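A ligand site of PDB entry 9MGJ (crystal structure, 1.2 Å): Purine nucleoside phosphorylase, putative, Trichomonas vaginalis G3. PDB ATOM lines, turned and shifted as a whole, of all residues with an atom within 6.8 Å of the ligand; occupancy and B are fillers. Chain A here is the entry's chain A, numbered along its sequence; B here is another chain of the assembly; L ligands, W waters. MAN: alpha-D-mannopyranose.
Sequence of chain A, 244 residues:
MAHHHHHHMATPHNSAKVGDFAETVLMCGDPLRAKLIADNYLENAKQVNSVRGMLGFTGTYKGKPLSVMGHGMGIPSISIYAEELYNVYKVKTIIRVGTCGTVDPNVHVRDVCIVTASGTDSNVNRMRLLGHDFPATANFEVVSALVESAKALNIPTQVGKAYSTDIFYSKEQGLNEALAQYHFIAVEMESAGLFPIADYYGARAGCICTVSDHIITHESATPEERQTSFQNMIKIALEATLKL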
ATOM      1  N   CYS A  28     -10.944  30.731  18.327  1.00  0.00           N
ATOM      2  CA  CYS A  28     -11.849  29.850  19.030  1.00  0.00           C
ATOM      3  C   CYS A  28     -11.004  29.035  19.997  1.00  0.00           C
ATOM      4  O   CYS A  28      -9.793  28.913  19.829  1.00  0.00           O
ATOM      5  CB  CYS A  28     -12.598  28.928  18.059  1.00  0.00           C
ATOM      6  SG  CYS A  28     -11.515  28.012  16.907  1.00  0.00           S
ATOM      7  N   GLY A  29     -11.641  28.443  21.002  1.00  0.00           N
ATOM      8  CA  GLY A  29     -10.864  27.722  22.006  1.00  0.00           C
ATOM      9  C   GLY A  29     -10.181  26.489  21.463  1.00  0.00           C
ATOM     10  O   GLY A  29      -9.054  26.185  21.844  1.00  0.00           O
ATOM     11  N   ASP A  30     -10.895  25.719  20.642  1.00  0.00           N
ATOM     12  CA  ASP A  30     -10.433  24.407  20.187  1.00  0.00           C
ATOM     13  C   ASP A  30      -9.578  24.574  18.947  1.00  0.00           C
ATOM     14  O   ASP A  30     -10.105  24.989  17.896  1.00  0.00           O
ATOM     15  CB  ASP A  30     -11.643  23.537  19.894  1.00  0.00           C
ATOM     16  CG  ASP A  30     -11.289  22.139  19.466  1.00  0.00           C
ATOM     17  OD1 ASP A  30     -10.094  21.845  19.302  1.00  0.00           O
ATOM     18  OD2 ASP A  30     -12.233  21.338  19.275  1.00  0.00           O
ATOM     19  N   ARG A  33     -11.009  23.103  15.874  1.00  0.00           N
ATOM     20  CA  ARG A  33     -12.038  23.900  15.234  1.00  0.00           C
ATOM     21  C   ARG A  33     -11.438  25.025  14.400  1.00  0.00           C
ATOM     22  O   ARG A  33     -11.978  25.370  13.351  1.00  0.00           O
ATOM     23  CB  ARG A  33     -12.998  24.460  16.293  1.00  0.00           C
ATOM     24  CG  ARG A  33     -14.156  25.262  15.697  1.00  0.00           C
ATOM     25  CD  ARG A  33     -15.400  25.235  16.599  1.00  0.00           C
ATOM     26  NE  ARG A  33     -15.896  23.872  16.799  1.00  0.00           N
ATOM     27  CZ  ARG A  33     -16.467  23.123  15.867  1.00  0.00           C
ATOM     28  NH1 ARG A  33     -16.636  23.579  14.631  1.00  0.00           N
ATOM     29  NH2 ARG A  33     -16.855  21.892  16.160  1.00  0.00           N
ATOM     30  N   HIS A  71      -7.289  29.428  20.886  1.00  0.00           N
ATOM     31  CA  HIS A  71      -6.839  30.175  22.056  1.00  0.00           C
ATOM     32  C   HIS A  71      -6.803  29.373  23.342  1.00  0.00           C
ATOM     33  O   HIS A  71      -6.394  29.927  24.368  1.00  0.00           O
ATOM     34  CB  HIS A  71      -7.590  31.513  22.251  1.00  0.00           C
ATOM     35  CG  HIS A  71      -9.078  31.399  22.453  1.00  0.00           C
ATOM     36  ND1 HIS A  71      -9.656  30.674  23.471  1.00  0.00           N
ATOM     37  CD2 HIS A  71     -10.101  31.999  21.792  1.00  0.00           C
ATOM     38  CE1 HIS A  71     -10.977  30.810  23.412  1.00  0.00           C
ATOM     39  NE2 HIS A  71     -11.265  31.595  22.394  1.00  0.00           N
ATOM     40  N   GLY A  72      -7.242  28.120  23.343  1.00  0.00           N
ATOM     41  CA  GLY A  72      -7.241  27.326  24.568  1.00  0.00           C
ATOM     42  C   GLY A  72      -8.368  27.750  25.492  1.00  0.00           C
ATOM     43  O   GLY A  72      -9.230  28.565  25.140  1.00  0.00           O
ATOM     44  N   MET A  73      -8.354  27.218  26.700  1.00  0.00           N
ATOM     45  CA  MET A  73      -9.444  27.455  27.648  1.00  0.00           C
ATOM     46  C   MET A  73      -8.991  28.345  28.780  1.00  0.00           C
ATOM     47  O   MET A  73      -7.996  28.058  29.452  1.00  0.00           O
ATOM     48  CB  MET A  73      -9.978  26.124  28.201  1.00  0.00           C
ATOM     49  CG  MET A  73     -10.525  25.218  27.094  1.00  0.00           C
ATOM     50  SD  MET A  73     -11.388  23.755  27.659  1.00  0.00           S
ATOM     51  CE  MET A  73     -10.056  22.981  28.552  1.00  0.00           C
ATOM     52  N   GLY A  74      -9.743  29.424  28.999  1.00  0.00           N
ATOM     53  CA  GLY A  74      -9.616  30.315  30.125  1.00  0.00           C
ATOM     54  C   GLY A  74      -8.862  31.588  29.820  1.00  0.00           C
ATOM     55  O   GLY A  74      -8.098  31.705  28.851  1.00  0.00           O
ATOM     56  N   ARG A  96     -13.452  36.713  18.876  1.00  0.00           N
ATOM     57  CA  ARG A  96     -13.584  35.401  19.486  1.00  0.00           C
ATOM     58  C   ARG A  96     -14.897  34.778  19.035  1.00  0.00           C
ATOM     59  O   ARG A  96     -15.952  35.415  19.079  1.00  0.00           O
ATOM     60  CB  ARG A  96     -13.539  35.509  21.014  1.00  0.00           C
ATOM     61  CG  ARG A  96     -13.739  34.193  21.685  1.00  0.00           C
ATOM     62  CD  ARG A  96     -13.461  34.224  23.186  1.00  0.00           C
ATOM     63  NE  ARG A  96     -14.534  33.530  23.889  1.00  0.00           N
ATOM     64  CZ  ARG A  96     -14.843  32.261  23.732  1.00  0.00           C
ATOM     65  NH1 ARG A  96     -14.162  31.481  22.921  1.00  0.00           N
ATOM     66  NH2 ARG A  96     -15.895  31.766  24.379  1.00  0.00           N
ATOM     67  N   VAL A  97     -14.823  33.531  18.601  1.00  0.00           N
ATOM     68  CA  VAL A  97     -15.978  32.766  18.142  1.00  0.00           C
ATOM     69  C   VAL A  97     -16.027  31.530  19.020  1.00  0.00           C
ATOM     70  O   VAL A  97     -15.076  30.755  19.068  1.00  0.00           O
ATOM     71  CB  VAL A  97     -15.878  32.428  16.650  1.00  0.00           C
ATOM     72  CG1 VAL A  97     -15.770  33.715  15.846  1.00  0.00           C
ATOM     73  CG2 VAL A  97     -14.711  31.557  16.333  1.00  0.00           C
ATOM     74  N   GLY A  98     -17.129  31.348  19.731  1.00  0.00           N
ATOM     75  CA  GLY A  98     -17.142  30.303  20.722  1.00  0.00           C
ATOM     76  C   GLY A  98     -18.499  29.713  20.969  1.00  0.00           C
ATOM     77  O   GLY A  98     -19.469  30.004  20.265  1.00  0.00           O
ATOM     78  N   THR A  99     -18.589  28.882  21.993  1.00  0.00           N
ATOM     79  CA  THR A  99     -19.829  28.346  22.489  1.00  0.00           C
ATOM     80  C   THR A  99     -19.986  28.830  23.914  1.00  0.00           C
ATOM     81  O   THR A  99     -19.014  29.232  24.562  1.00  0.00           O
ATOM     82  CB  THR A  99     -19.848  26.811  22.443  1.00  0.00           C
ATOM     83  OG1 THR A  99     -18.885  26.278  23.374  1.00  0.00           O
ATOM     84  CG2 THR A  99     -19.499  26.314  21.045  1.00  0.00           C
ATOM     85  N   CYS A 100     -21.207  28.773  24.413  1.00  0.00           N
ATOM     86  CA  CYS A 100     -21.484  29.266  25.746  1.00  0.00           C
ATOM     87  C   CYS A 100     -22.678  28.541  26.338  1.00  0.00           C
ATOM     88  O   CYS A 100     -23.439  27.887  25.638  1.00  0.00           O
ATOM     89  CB  CYS A 100     -21.744  30.788  25.741  1.00  0.00           C
ATOM     90  SG  CYS A 100     -23.239  31.280  24.858  1.00  0.00           S
ATOM     91  N   PHE A 168     -15.027  26.283  35.228  1.00  0.00           N
ATOM     92  CA  PHE A 168     -16.049  25.543  34.497  1.00  0.00           C
ATOM     93  C   PHE A 168     -16.949  24.773  35.454  1.00  0.00           C
ATOM     94  O   PHE A 168     -18.178  24.778  35.307  1.00  0.00           O
ATOM     95  CB  PHE A 168     -15.353  24.608  33.526  1.00  0.00           C
ATOM     96  CG  PHE A 168     -16.277  23.880  32.591  1.00  0.00           C
ATOM     97  CD1 PHE A 168     -16.882  22.688  32.961  1.00  0.00           C
ATOM     98  CD2 PHE A 168     -16.550  24.387  31.331  1.00  0.00           C
ATOM     99  CE1 PHE A 168     -17.731  22.028  32.108  1.00  0.00           C
ATOM    100  CE2 PHE A 168     -17.393  23.712  30.462  1.00  0.00           C
ATOM    101  CZ  PHE A 168     -17.997  22.546  30.859  1.00  0.00           C
ATOM    102  N   VAL A 187     -22.576  32.592  29.236  1.00  0.00           N
ATOM    103  CA  VAL A 187     -21.599  32.209  30.237  1.00  0.00           C
ATOM    104  C   VAL A 187     -20.505  31.443  29.509  1.00  0.00           C
ATOM    105  O   VAL A 187     -20.776  30.403  28.888  1.00  0.00           O
ATOM    106  CB  VAL A 187     -22.220  31.353  31.356  1.00  0.00           C
ATOM    107  CG1 VAL A 187     -21.172  31.014  32.404  1.00  0.00           C
ATOM    108  CG2 VAL A 187     -23.410  32.079  31.995  1.00  0.00           C
ATOM    109  N   GLU A 188     -19.284  31.945  29.588  1.00  0.00           N
ATOM    110  CA  GLU A 188     -18.137  31.346  28.884  1.00  0.00           C
ATOM    111  C   GLU A 188     -16.903  31.617  29.748  1.00  0.00           C
ATOM    112  O   GLU A 188     -17.036  31.869  30.949  1.00  0.00           O
ATOM    113  CB  GLU A 188     -18.071  31.783  27.413  1.00  0.00           C
ATOM    114  CG  GLU A 188     -18.224  33.253  27.164  1.00  0.00           C
ATOM    115  CD  GLU A 188     -16.947  34.048  27.325  1.00  0.00           C
ATOM    116  OE1 GLU A 188     -15.933  33.712  26.665  1.00  0.00           O
ATOM    117  OE2 GLU A 188     -16.940  34.980  28.123  1.00  0.00           O
ATOM    118  N   MET A 189     -15.707  31.504  29.180  1.00  0.00           N
ATOM    119  CA  MET A 189     -14.495  31.522  30.001  1.00  0.00           C
ATOM    120  C   MET A 189     -13.383  32.466  29.533  1.00  0.00           C
ATOM    121  O   MET A 189     -12.365  32.536  30.236  1.00  0.00           O
ATOM    122  CB  MET A 189     -13.925  30.100  30.206  1.00  0.00           C
ATOM    123  CG  MET A 189     -14.899  29.183  30.843  1.00  0.00           C
ATOM    124  SD  MET A 189     -14.214  27.543  31.186  1.00  0.00           S
ATOM    125  CE  MET A 189     -12.930  27.927  32.384  1.00  0.00           C
ATOM    126  N   GLU A 190     -13.528  33.183  28.407  1.00  0.00           N
ATOM    127  CA  GLU A 190     -12.390  33.918  27.863  1.00  0.00           C
ATOM    128  C   GLU A 190     -12.585  35.392  27.522  1.00  0.00           C
ATOM    129  O   GLU A 190     -11.609  36.148  27.580  1.00  0.00           O
ATOM    130  CB  GLU A 190     -11.866  33.233  26.584  1.00  0.00           C
ATOM    131  CG  GLU A 190     -11.258  31.873  26.809  1.00  0.00           C
ATOM    132  CD  GLU A 190     -12.279  30.754  26.761  1.00  0.00           C
ATOM    133  OE1 GLU A 190     -13.294  30.905  26.036  1.00  0.00           O
ATOM    134  OE2 GLU A 190     -12.011  29.706  27.402  1.00  0.00           O
ATOM    135  N   SER A 191     -13.790  35.805  27.130  1.00  0.00           N
ATOM    136  CA  SER A 191     -13.908  37.129  26.506  1.00  0.00           C
ATOM    137  C   SER A 191     -13.503  38.273  27.424  1.00  0.00           C
ATOM    138  O   SER A 191     -12.924  39.263  26.946  1.00  0.00           O
ATOM    139  CB  SER A 191     -15.305  37.346  25.921  1.00  0.00           C
ATOM    140  OG  SER A 191     -16.295  37.400  26.910  1.00  0.00           O
ATOM    141  N   CYS A 209     -20.936  33.987  20.317  1.00  0.00           N
ATOM    142  CA  CYS A 209     -21.019  32.615  20.817  1.00  0.00           C
ATOM    143  C   CYS A 209     -22.376  32.027  20.479  1.00  0.00           C
ATOM    144  O   CYS A 209     -23.358  32.735  20.375  1.00  0.00           O
ATOM    145  CB  CYS A 209     -20.906  32.552  22.346  1.00  0.00           C
ATOM    146  SG  CYS A 209     -19.316  33.001  23.043  1.00  0.00           S
ATOM    147  N   SER A 212     -24.767  26.333  23.685  1.00  0.00           N
ATOM    148  CA  SER A 212     -24.770  24.881  23.638  1.00  0.00           C
ATOM    149  C   SER A 212     -25.621  24.254  24.725  1.00  0.00           C
ATOM    150  O   SER A 212     -26.121  23.144  24.550  1.00  0.00           O
ATOM    151  CB  SER A 212     -23.336  24.342  23.721  1.00  0.00           C
ATOM    152  OG  SER A 212     -22.731  24.693  24.953  1.00  0.00           O
ATOM    153  N   MET A 233     -23.094  30.910  13.163  1.00  0.00           N
ATOM    154  CA  MET A 233     -22.210  31.859  13.829  1.00  0.00           C
ATOM    155  C   MET A 233     -20.979  32.168  13.002  1.00  0.00           C
ATOM    156  O   MET A 233     -20.579  33.325  12.888  1.00  0.00           O
ATOM    157  CB  MET A 233     -21.798  31.321  15.200  1.00  0.00           C
ATOM    158  CG  MET A 233     -20.584  32.030  15.777  1.00  0.00           C
ATOM    159  SD  MET A 233     -20.149  31.480  17.424  1.00  0.00           S
ATOM    160  CE  MET A 233     -19.676  29.798  17.119  1.00  0.00           C
ATOM    161  N   HIS B  13     -14.537  17.420  27.572  1.00  0.00           N
ATOM    162  CA  HIS B  13     -13.182  17.771  27.166  1.00  0.00           C
ATOM    163  C   HIS B  13     -12.288  16.554  27.024  1.00  0.00           C
ATOM    164  O   HIS B  13     -11.078  16.711  26.782  1.00  0.00           O
ATOM    165  CB  HIS B  13     -12.564  18.750  28.171  1.00  0.00           C
ATOM    166  CG  HIS B  13     -13.470  19.893  28.490  1.00  0.00           C
ATOM    167  ND1 HIS B  13     -14.205  19.939  29.657  1.00  0.00           N
ATOM    168  CD2 HIS B  13     -13.781  21.023  27.806  1.00  0.00           C
ATOM    169  CE1 HIS B  13     -14.937  21.049  29.665  1.00  0.00           C
ATOM    170  NE2 HIS B  13     -14.701  21.722  28.546  1.00  0.00           N
ATOM    171  N   ARG B  52      -9.651  18.579  21.562  1.00  0.00           N
ATOM    172  CA  ARG B  52      -8.964  19.863  21.585  1.00  0.00           C
ATOM    173  C   ARG B  52      -7.457  19.737  21.392  1.00  0.00           C
ATOM    174  O   ARG B  52      -6.713  20.661  21.714  1.00  0.00           O
ATOM    175  CB  ARG B  52      -9.307  20.720  22.823  1.00  0.00           C
ATOM    176  CG  ARG B  52     -10.756  21.117  22.872  1.00  0.00           C
ATOM    177  CD  ARG B  52     -11.166  21.520  24.265  1.00  0.00           C
ATOM    178  NE  ARG B  52     -12.539  21.982  24.295  1.00  0.00           N
ATOM    179  CZ  ARG B  52     -12.907  23.252  24.217  1.00  0.00           C
ATOM    180  NH1 ARG B  52     -12.018  24.228  24.058  1.00  0.00           N
ATOM    181  NH2 ARG B  52     -14.193  23.555  24.299  1.00  0.00           N
ATOM    182  N   ILE B  80     -10.121  22.413  34.709  1.00  0.00           N
ATOM    183  CA  ILE B  80     -11.030  21.559  33.963  1.00  0.00           C
ATOM    184  C   ILE B  80     -10.473  20.140  33.898  1.00  0.00           C
ATOM    185  O   ILE B  80     -11.153  19.167  34.235  1.00  0.00           O
ATOM    186  CB  ILE B  80     -11.246  22.119  32.547  1.00  0.00           C
ATOM    187  CG1 ILE B  80     -12.176  23.318  32.601  1.00  0.00           C
ATOM    188  CG2 ILE B  80     -11.822  21.065  31.598  1.00  0.00           C
ATOM    189  CD1 ILE B  80     -12.148  24.178  31.377  1.00  0.00           C
HETATM  190  C1  MAN L   1     -15.246  26.074  26.798  1.00  0.00           C
HETATM  191  C2  MAN L   1     -14.834  27.475  27.204  1.00  0.00           C
HETATM  192  C3  MAN L   1     -15.725  28.467  26.470  1.00  0.00           C
HETATM  193  C4  MAN L   1     -15.577  28.267  24.953  1.00  0.00           C
HETATM  194  C5  MAN L   1     -15.848  26.824  24.546  1.00  0.00           C
HETATM  195  C6  MAN L   1     -15.344  26.434  23.161  1.00  0.00           C
HETATM  196  O1  MAN L   1     -16.530  25.839  27.254  1.00  0.00           O
HETATM  197  O2  MAN L   1     -13.492  27.621  26.827  1.00  0.00           O
HETATM  198  O3  MAN L   1     -15.384  29.775  26.886  1.00  0.00           O
HETATM  199  O4  MAN L   1     -16.500  29.093  24.275  1.00  0.00           O
HETATM  200  O5  MAN L   1     -15.143  25.937  25.413  1.00  0.00           O
HETATM  201  O6  MAN L   1     -15.955  27.133  22.116  1.00  0.00           O
HETATM  202  O   HOH W   1     -15.688  24.084  20.598  1.00  0.00           O
HETATM  203  O   HOH W   2     -13.918  26.099  19.823  1.00  0.00           O
HETATM  204  O   HOH W   3     -12.482  27.101  24.640  1.00  0.00           O
HETATM  205  O   HOH W   4     -16.731  23.151  27.176  1.00  0.00           O
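The backbone NH (N) of Met 189 sits at hydrogen-bond distance from an oxygen (O3) of the ligand (2.9 Å). OE1 of Glu 190 is in hydrogen-bond range of O3 of the ligand. An oxygen (O4) of the ligand lies within hydrogen-bond range of the guanidinium group (NH2) of Arg 96, 2.7 Å away. The backbone NH (N) of Thr 99 is in hydrogen-bond range of an oxygen (O4) of the ligand, at 3.1 Å. O5 of the ligand sits at hydrogen-bond distance from NH2 of Arg 52 of chain B (2.8 Å). The backbone carbonyl oxygen of Thr 99 is in hydrogen-bond range of an oxygen (O4) of the ligand (2.5 Å). An oxygen (O6) of the ligand lies close to the side-chain hydroxyl of Thr 99 (3.3 Å).
The side-chain carboxylate (OE1) of Glu 188 is in salt-bridge range of the guanidinium group (NH2) of Arg 96 (3.0 Å). SD of Met 73 sits close to NH1 of Arg 52 of chain B (3.7 Å). The backbone NH (N) of Glu 190 sits at hydrogen-bond distance from the side-chain carboxylate (OE1) of Glu 188. The guanidinium group of Arg 96 sits at hydrogen-bond distance from a ring nitrogen (NE2) of His 71 (2.9 Å). N of Gly 74 lies within hydrogen-bond range of OE2 of Glu 190 (2.8 Å). NH2 of Arg 96 lies within salt-bridge range of OE1 of Glu 190 (3.2 Å). OE2 of Glu 188 is in hydrogen-bond range of OG of Ser 191 (2.8 Å).
Met 73 touches the ligand. CA of Gly 98 touches O6 of the ligand (3.7 Å). Phe 168 touches the ligand. CB of Glu 188 touches O3 of the ligand, 3.4 Å away. Hydrophobic or aromatic side chains within 4 Å of the ligand: Met 73, Phe 168 and Met 189. Of the 25 residues printed, 9 come within 4 Å of the ligand.
Water W3 lies within hydrogen-bond range of an oxygen (O2) of the ligand (2.5 Å) and the guanidinium group of Arg 52 of chain B (3.0 Å). Water W4 lies within hydrogen-bond range of an oxygen (O1) of the ligand and a ring nitrogen (NE2) of His 13 of chain B. Water W2 lies within hydrogen-bond range of the backbone NH (N) of Asp 30 (3.2 Å), an oxygen (O6) of the ligand (3.2 Å) and the backbone NH (N) of Gly 29 (3.5 Å).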
